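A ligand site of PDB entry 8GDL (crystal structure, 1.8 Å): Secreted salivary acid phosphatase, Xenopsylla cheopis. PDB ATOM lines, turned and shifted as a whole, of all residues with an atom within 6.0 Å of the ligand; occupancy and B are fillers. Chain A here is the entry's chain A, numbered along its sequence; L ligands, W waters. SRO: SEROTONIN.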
ATOM      1  N   VAL A  11      25.971  20.361 -10.564  1.00  0.00           N
ATOM      2  CA  VAL A  11      24.553  20.700 -10.445  1.00  0.00           C
ATOM      3  C   VAL A  11      23.917  20.716 -11.825  1.00  0.00           C
ATOM      4  O   VAL A  11      24.466  21.309 -12.765  1.00  0.00           O
ATOM      5  CB  VAL A  11      24.329  22.064  -9.757  1.00  0.00           C
ATOM      6  CG1 VAL A  11      22.838  22.344  -9.644  1.00  0.00           C
ATOM      7  CG2 VAL A  11      24.978  22.089  -8.392  1.00  0.00           C
ATOM      8  N   PHE A  12      22.758  20.061 -11.942  1.00  0.00           N
ATOM      9  CA  PHE A  12      21.841  20.272 -13.057  1.00  0.00           C
ATOM     10  C   PHE A  12      20.733  21.209 -12.596  1.00  0.00           C
ATOM     11  O   PHE A  12      20.169  21.020 -11.512  1.00  0.00           O
ATOM     12  CB  PHE A  12      21.164  18.978 -13.529  1.00  0.00           C
ATOM     13  CG  PHE A  12      22.083  17.840 -13.889  1.00  0.00           C
ATOM     14  CD1 PHE A  12      22.618  17.031 -12.897  1.00  0.00           C
ATOM     15  CD2 PHE A  12      22.286  17.501 -15.225  1.00  0.00           C
ATOM     16  CE1 PHE A  12      23.413  15.929 -13.227  1.00  0.00           C
ATOM     17  CE2 PHE A  12      23.075  16.424 -15.571  1.00  0.00           C
ATOM     18  CZ  PHE A  12      23.641  15.629 -14.567  1.00  0.00           C
ATOM     19  N   VAL A  13      20.396  22.197 -13.425  1.00  0.00           N
ATOM     20  CA  VAL A  13      19.244  23.067 -13.205  1.00  0.00           C
ATOM     21  C   VAL A  13      18.327  22.936 -14.420  1.00  0.00           C
ATOM     22  O   VAL A  13      18.819  23.012 -15.560  1.00  0.00           O
ATOM     23  CB  VAL A  13      19.652  24.540 -12.993  1.00  0.00           C
ATOM     24  CG1 VAL A  13      18.394  25.434 -12.845  1.00  0.00           C
ATOM     25  CG2 VAL A  13      20.534  24.702 -11.772  1.00  0.00           C
ATOM     26  N   MET A  14      17.016  22.755 -14.207  1.00  0.00           N
ATOM     27  CA  MET A  14      16.094  23.008 -15.313  1.00  0.00           C
ATOM     28  C   MET A  14      15.156  24.121 -14.889  1.00  0.00           C
ATOM     29  O   MET A  14      14.561  24.073 -13.799  1.00  0.00           O
ATOM     30  CB  MET A  14      15.338  21.749 -15.793  1.00  0.00           C
ATOM     31  CG  MET A  14      13.890  21.951 -16.334  1.00  0.00           C
ATOM     32  SD  MET A  14      12.843  20.508 -16.554  1.00  0.00           S
ATOM     33  CE  MET A  14      13.776  19.450 -17.668  1.00  0.00           C
ATOM     34  N   TRP A  75      27.256  24.897 -18.844  1.00  0.00           N
ATOM     35  CA  TRP A  75      26.690  24.497 -20.125  1.00  0.00           C
ATOM     36  C   TRP A  75      25.253  24.969 -20.209  1.00  0.00           C
ATOM     37  O   TRP A  75      24.361  24.376 -19.590  1.00  0.00           O
ATOM     38  CB  TRP A  75      26.767  22.986 -20.283  1.00  0.00           C
ATOM     39  CG  TRP A  75      26.367  22.470 -21.602  1.00  0.00           C
ATOM     40  CD1 TRP A  75      26.212  23.179 -22.769  1.00  0.00           C
ATOM     41  CD2 TRP A  75      26.091  21.110 -21.916  1.00  0.00           C
ATOM     42  NE1 TRP A  75      25.847  22.328 -23.790  1.00  0.00           N
ATOM     43  CE2 TRP A  75      25.776  21.042 -23.290  1.00  0.00           C
ATOM     44  CE3 TRP A  75      26.092  19.921 -21.159  1.00  0.00           C
ATOM     45  CZ2 TRP A  75      25.448  19.851 -23.926  1.00  0.00           C
ATOM     46  CZ3 TRP A  75      25.774  18.732 -21.797  1.00  0.00           C
ATOM     47  CH2 TRP A  75      25.451  18.712 -23.166  1.00  0.00           C
ATOM     48  N   VAL A  77      21.778  25.116 -22.057  1.00  0.00           N
ATOM     49  CA  VAL A  77      21.057  24.386 -23.071  1.00  0.00           C
ATOM     50  C   VAL A  77      19.586  24.801 -23.022  1.00  0.00           C
ATOM     51  O   VAL A  77      19.122  25.414 -22.067  1.00  0.00           O
ATOM     52  CB  VAL A  77      21.213  22.850 -22.918  1.00  0.00           C
ATOM     53  CG1 VAL A  77      22.639  22.454 -23.263  1.00  0.00           C
ATOM     54  CG2 VAL A  77      20.898  22.426 -21.501  1.00  0.00           C
ATOM     55  N   PHE A 116      21.476  19.680 -27.050  1.00  0.00           N
ATOM     56  CA  PHE A 116      22.153  18.461 -26.680  1.00  0.00           C
ATOM     57  C   PHE A 116      21.399  17.305 -27.323  1.00  0.00           C
ATOM     58  O   PHE A 116      20.266  17.475 -27.772  1.00  0.00           O
ATOM     59  CB  PHE A 116      22.252  18.297 -25.149  1.00  0.00           C
ATOM     60  CG  PHE A 116      20.939  18.305 -24.450  1.00  0.00           C
ATOM     61  CD1 PHE A 116      20.296  19.507 -24.155  1.00  0.00           C
ATOM     62  CD2 PHE A 116      20.347  17.109 -24.060  1.00  0.00           C
ATOM     63  CE1 PHE A 116      19.091  19.502 -23.499  1.00  0.00           C
ATOM     64  CE2 PHE A 116      19.141  17.098 -23.412  1.00  0.00           C
ATOM     65  CZ  PHE A 116      18.507  18.305 -23.132  1.00  0.00           C
ATOM     66  N   ALA A 118      19.792  14.341 -26.646  1.00  0.00           N
ATOM     67  CA  ALA A 118      18.473  13.857 -26.260  1.00  0.00           C
ATOM     68  C   ALA A 118      17.395  14.926 -26.232  1.00  0.00           C
ATOM     69  O   ALA A 118      16.227  14.587 -25.981  1.00  0.00           O
ATOM     70  CB  ALA A 118      18.519  13.182 -24.885  1.00  0.00           C
ATOM     71  N   PHE A 122      12.741  14.742 -25.796  1.00  0.00           N
ATOM     72  CA  PHE A 122      11.962  15.142 -24.632  1.00  0.00           C
ATOM     73  C   PHE A 122      10.583  15.701 -25.002  1.00  0.00           C
ATOM     74  O   PHE A 122       9.670  15.692 -24.163  1.00  0.00           O
ATOM     75  CB  PHE A 122      12.753  16.201 -23.833  1.00  0.00           C
ATOM     76  CG  PHE A 122      14.027  15.694 -23.208  1.00  0.00           C
ATOM     77  CD1 PHE A 122      14.316  14.328 -23.146  1.00  0.00           C
ATOM     78  CD2 PHE A 122      14.941  16.599 -22.659  1.00  0.00           C
ATOM     79  CE1 PHE A 122      15.498  13.866 -22.546  1.00  0.00           C
ATOM     80  CE2 PHE A 122      16.124  16.135 -22.046  1.00  0.00           C
ATOM     81  CZ  PHE A 122      16.392  14.768 -21.995  1.00  0.00           C
ATOM     82  N   LEU A 228      12.354   9.631 -20.502  1.00  0.00           N
ATOM     83  CA  LEU A 228      13.569   9.985 -21.205  1.00  0.00           C
ATOM     84  C   LEU A 228      14.401  10.971 -20.420  1.00  0.00           C
ATOM     85  O   LEU A 228      15.612  11.042 -20.595  1.00  0.00           O
ATOM     86  CB  LEU A 228      13.262  10.549 -22.595  1.00  0.00           C
ATOM     87  CG  LEU A 228      12.554   9.633 -23.584  1.00  0.00           C
ATOM     88  CD1 LEU A 228      12.135  10.484 -24.785  1.00  0.00           C
ATOM     89  CD2 LEU A 228      13.435   8.472 -24.022  1.00  0.00           C
ATOM     90  N   LEU A 229      13.753  11.787 -19.589  1.00  0.00           N
ATOM     91  CA  LEU A 229      14.492  12.709 -18.735  1.00  0.00           C
ATOM     92  C   LEU A 229      15.357  11.932 -17.765  1.00  0.00           C
ATOM     93  O   LEU A 229      16.560  12.190 -17.643  1.00  0.00           O
ATOM     94  CB  LEU A 229      13.525  13.609 -17.970  1.00  0.00           C
ATOM     95  CG  LEU A 229      12.603  14.439 -18.854  1.00  0.00           C
ATOM     96  CD1 LEU A 229      11.642  15.205 -17.978  1.00  0.00           C
ATOM     97  CD2 LEU A 229      13.480  15.360 -19.636  1.00  0.00           C
ATOM     98  N   LEU A 230      14.752  10.964 -17.069  1.00  0.00           N
ATOM     99  CA  LEU A 230      15.511  10.074 -16.177  1.00  0.00           C
ATOM    100  C   LEU A 230      16.637   9.398 -16.938  1.00  0.00           C
ATOM    101  O   LEU A 230      17.785   9.391 -16.488  1.00  0.00           O
ATOM    102  CB  LEU A 230      14.579   9.037 -15.556  1.00  0.00           C
ATOM    103  CG  LEU A 230      13.467   9.647 -14.693  1.00  0.00           C
ATOM    104  CD1 LEU A 230      12.509   8.582 -14.220  1.00  0.00           C
ATOM    105  CD2 LEU A 230      14.031  10.415 -13.519  1.00  0.00           C
ATOM    106  N   ASP A 232      18.316  10.191 -19.645  1.00  0.00           N
ATOM    107  CA  ASP A 232      19.463  11.012 -20.004  1.00  0.00           C
ATOM    108  C   ASP A 232      20.219  11.474 -18.758  1.00  0.00           C
ATOM    109  O   ASP A 232      21.458  11.530 -18.757  1.00  0.00           O
ATOM    110  CB  ASP A 232      19.030  12.210 -20.845  1.00  0.00           C
ATOM    111  CG  ASP A 232      20.160  12.746 -21.722  1.00  0.00           C
ATOM    112  OD1 ASP A 232      20.908  11.914 -22.296  1.00  0.00           O
ATOM    113  OD2 ASP A 232      20.269  13.978 -21.867  1.00  0.00           O
ATOM    114  N   LEU A 233      19.497  11.811 -17.698  1.00  0.00           N
ATOM    115  CA  LEU A 233      20.144  12.191 -16.443  1.00  0.00           C
ATOM    116  C   LEU A 233      21.066  11.090 -15.945  1.00  0.00           C
ATOM    117  O   LEU A 233      22.205  11.344 -15.556  1.00  0.00           O
ATOM    118  CB  LEU A 233      19.116  12.524 -15.382  1.00  0.00           C
ATOM    119  CG  LEU A 233      18.502  13.927 -15.526  1.00  0.00           C
ATOM    120  CD1 LEU A 233      17.383  14.149 -14.509  1.00  0.00           C
ATOM    121  CD2 LEU A 233      19.564  14.988 -15.418  1.00  0.00           C
ATOM    122  N   ASP A 236      24.225  10.692 -17.926  1.00  0.00           N
ATOM    123  CA  ASP A 236      25.198  11.691 -17.500  1.00  0.00           C
ATOM    124  C   ASP A 236      25.781  11.359 -16.140  1.00  0.00           C
ATOM    125  O   ASP A 236      27.008  11.399 -15.950  1.00  0.00           O
ATOM    126  CB  ASP A 236      24.534  13.072 -17.450  1.00  0.00           C
ATOM    127  CG  ASP A 236      24.319  13.670 -18.805  1.00  0.00           C
ATOM    128  OD1 ASP A 236      24.730  13.073 -19.828  1.00  0.00           O
ATOM    129  OD2 ASP A 236      23.710  14.749 -18.849  1.00  0.00           O
ATOM    130  N   GLN A 246      30.692  15.187 -17.784  1.00  0.00           N
ATOM    131  CA  GLN A 246      29.344  15.050 -18.289  1.00  0.00           C
ATOM    132  C   GLN A 246      29.407  14.744 -19.784  1.00  0.00           C
ATOM    133  O   GLN A 246      30.149  15.408 -20.516  1.00  0.00           O
ATOM    134  CB  GLN A 246      28.548  16.340 -18.044  1.00  0.00           C
ATOM    135  CG  GLN A 246      27.131  16.288 -18.577  1.00  0.00           C
ATOM    136  CD  GLN A 246      26.370  17.602 -18.421  1.00  0.00           C
ATOM    137  OE1 GLN A 246      26.945  18.671 -18.204  1.00  0.00           O
ATOM    138  NE2 GLN A 246      25.047  17.512 -18.480  1.00  0.00           N
ATOM    139  N   ASN A 258      25.044  22.577 -15.416  1.00  0.00           N
ATOM    140  CA  ASN A 258      24.260  22.442 -16.633  1.00  0.00           C
ATOM    141  C   ASN A 258      22.931  23.154 -16.401  1.00  0.00           C
ATOM    142  O   ASN A 258      22.227  22.861 -15.423  1.00  0.00           O
ATOM    143  CB  ASN A 258      24.083  20.960 -16.968  1.00  0.00           C
ATOM    144  CG  ASN A 258      23.559  20.697 -18.374  1.00  0.00           C
ATOM    145  OD1 ASN A 258      23.165  19.574 -18.670  1.00  0.00           O
ATOM    146  ND2 ASN A 258      23.527  21.725 -19.240  1.00  0.00           N
ATOM    147  N   VAL A 259      22.596  24.117 -17.249  1.00  0.00           N
ATOM    148  CA  VAL A 259      21.372  24.892 -17.073  1.00  0.00           C
ATOM    149  C   VAL A 259      20.510  24.655 -18.305  1.00  0.00           C
ATOM    150  O   VAL A 259      20.919  25.021 -19.414  1.00  0.00           O
ATOM    151  CB  VAL A 259      21.656  26.395 -16.899  1.00  0.00           C
ATOM    152  CG1 VAL A 259      20.338  27.158 -16.819  1.00  0.00           C
ATOM    153  CG2 VAL A 259      22.468  26.648 -15.640  1.00  0.00           C
ATOM    154  N   PHE A 260      19.325  24.068 -18.095  1.00  0.00           N
ATOM    155  CA  PHE A 260      18.414  23.642 -19.168  1.00  0.00           C
ATOM    156  C   PHE A 260      17.136  24.481 -19.079  1.00  0.00           C
ATOM    157  O   PHE A 260      16.324  24.286 -18.172  1.00  0.00           O
ATOM    158  CB  PHE A 260      18.103  22.153 -19.005  1.00  0.00           C
ATOM    159  CG  PHE A 260      17.239  21.552 -20.085  1.00  0.00           C
ATOM    160  CD1 PHE A 260      17.090  22.154 -21.326  1.00  0.00           C
ATOM    161  CD2 PHE A 260      16.619  20.331 -19.856  1.00  0.00           C
ATOM    162  CE1 PHE A 260      16.302  21.548 -22.311  1.00  0.00           C
ATOM    163  CE2 PHE A 260      15.841  19.732 -20.834  1.00  0.00           C
ATOM    164  CZ  PHE A 260      15.673  20.342 -22.055  1.00  0.00           C
ATOM    165  N   GLN A 270       9.364  16.829 -15.464  1.00  0.00           N
ATOM    166  CA  GLN A 270      10.547  16.538 -14.654  1.00  0.00           C
ATOM    167  C   GLN A 270      10.201  16.366 -13.172  1.00  0.00           C
ATOM    168  O   GLN A 270      10.735  15.475 -12.497  1.00  0.00           O
ATOM    169  CB  GLN A 270      11.569  17.667 -14.825  1.00  0.00           C
ATOM    170  CG  GLN A 270      12.909  17.457 -14.121  1.00  0.00           C
ATOM    171  CD  GLN A 270      13.637  16.197 -14.596  1.00  0.00           C
ATOM    172  OE1 GLN A 270      14.494  16.267 -15.471  1.00  0.00           O
ATOM    173  NE2 GLN A 270      13.265  15.050 -14.044  1.00  0.00           N
ATOM    174  N   VAL A 299      14.027  23.358 -11.078  1.00  0.00           N
ATOM    175  CA  VAL A 299      14.396  22.148 -10.346  1.00  0.00           C
ATOM    176  C   VAL A 299      15.912  22.059 -10.357  1.00  0.00           C
ATOM    177  O   VAL A 299      16.533  22.151 -11.428  1.00  0.00           O
ATOM    178  CB  VAL A 299      13.759  20.904 -10.983  1.00  0.00           C
ATOM    179  CG1 VAL A 299      14.238  19.613 -10.287  1.00  0.00           C
ATOM    180  CG2 VAL A 299      12.250  20.978 -10.939  1.00  0.00           C
ATOM    181  N   ILE A 301      19.284  19.778  -9.271  1.00  0.00           N
ATOM    182  CA  ILE A 301      19.744  18.416  -9.003  1.00  0.00           C
ATOM    183  C   ILE A 301      21.197  18.562  -8.545  1.00  0.00           C
ATOM    184  O   ILE A 301      22.091  18.776  -9.359  1.00  0.00           O
ATOM    185  CB  ILE A 301      19.636  17.542 -10.257  1.00  0.00           C
ATOM    186  CG1 ILE A 301      18.208  17.599 -10.824  1.00  0.00           C
ATOM    187  CG2 ILE A 301      20.023  16.097  -9.957  1.00  0.00           C
ATOM    188  CD1 ILE A 301      18.098  17.129 -12.280  1.00  0.00           C
HETATM  189  OH  SRO L   1      20.167  20.929 -16.563  1.00  0.00           O
HETATM  190  CZ3 SRO L   1      19.310  19.841 -16.698  1.00  0.00           C
HETATM  191  CH2 SRO L   1      18.290  19.699 -15.758  1.00  0.00           C
HETATM  192  CZ2 SRO L   1      17.431  18.618 -15.825  1.00  0.00           C
HETATM  193  CE2 SRO L   1      17.574  17.693 -16.877  1.00  0.00           C
HETATM  194  NE1 SRO L   1      16.879  16.563 -17.217  1.00  0.00           N
HETATM  195  CD1 SRO L   1      17.456  16.014 -18.325  1.00  0.00           C
HETATM  196  CG  SRO L   1      18.498  16.839 -18.695  1.00  0.00           C
HETATM  197  CD2 SRO L   1      18.576  17.842 -17.797  1.00  0.00           C
HETATM  198  CE3 SRO L   1      19.455  18.933 -17.724  1.00  0.00           C
HETATM  199  CB  SRO L   1      19.391  16.533 -19.888  1.00  0.00           C
HETATM  200  CA  SRO L   1      20.725  16.013 -19.364  1.00  0.00           C
HETATM  201  NZ  SRO L   1      21.588  15.684 -20.505  1.00  0.00           N
HETATM  202  O   HOH W   1      24.632  15.312 -21.677  1.00  0.00           O
HETATM  203  O   HOH W   2      22.486  18.511 -20.853  1.00  0.00           O
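OD2 of Asp 232 is in salt-bridge range of NZ of the ligand (2.6 Å). An oxygen (OH) of the ligand is in hydrogen-bond range of the backbone NH of Val 13, at 3.4 Å. An oxygen (OH) of the ligand lies within hydrogen-bond range of the backbone carbonyl oxygen of Val 13 (2.7 Å). A nitrogen (NZ) of the ligand is in salt-bridge range of the side-chain carboxylate (OD2) of Asp 236, at 2.8 Å. The side-chain amide oxygen of Gln 270 lies within hydrogen-bond range of a nitrogen (NE1) of the ligand (3.0 Å). O of Asn 258 sits at hydrogen-bond distance from OH of the ligand (3.0 Å).
Water W2 lies within hydrogen-bond range of OD1 of Asn 258 and NZ of the ligand. Water W1 lies within hydrogen-bond range of the side-chain carboxylate (OD1) of Asp 236 and a nitrogen (NZ) of the ligand.
Phe 12 touches the ligand. Met 14 touches the ligand (CB to CH2, 3.6 Å). Phe 116 touches the ligand (CE2 to CB, 3.6 Å). Phe 122 touches the ligand. O of Leu 229 touches CD1 of the ligand (3.99 Å). Leu 233 touches the ligand. Phe 260 touches the ligand. Ile 301 touches the ligand (CD1 to CZ2, 3.9 Å). Of the 22 residues printed, 13 come within 4 Å of the ligand.
The backbone NH (N) of Val 13 is in hydrogen-bond range of the backbone carbonyl oxygen (O) of Asn 258 (2.8 Å). O of Val 13 sits at hydrogen-bond distance from N of Phe 260 (2.8 Å). The side-chain amide nitrogen (NE2) of Gln 246 is in hydrogen-bond range of the side-chain carboxylate (OD2) of Asp 236. The side-chain amide oxygen (OD1) of Asn 258 lies within hydrogen-bond range of the side-chain amide nitrogen (NE2) of Gln 246 (2.8 Å). The backbone carbonyl oxygen (O) of Trp 75 lies within hydrogen-bond range of the side-chain amide nitrogen (ND2) of Asn 258 (2.8 Å). N of Asn 258 is in hydrogen-bond range of O of Val 11 (3.0 Å). The backbone carbonyl oxygen (O) of Met 14 lies within hydrogen-bond range of the backbone NH (N) of Val 299 (2.9 Å). The backbone NH (N) of Ile 301 sits at hydrogen-bond distance from the backbone carbonyl oxygen (O) of Phe 12, 2.7 Å away.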
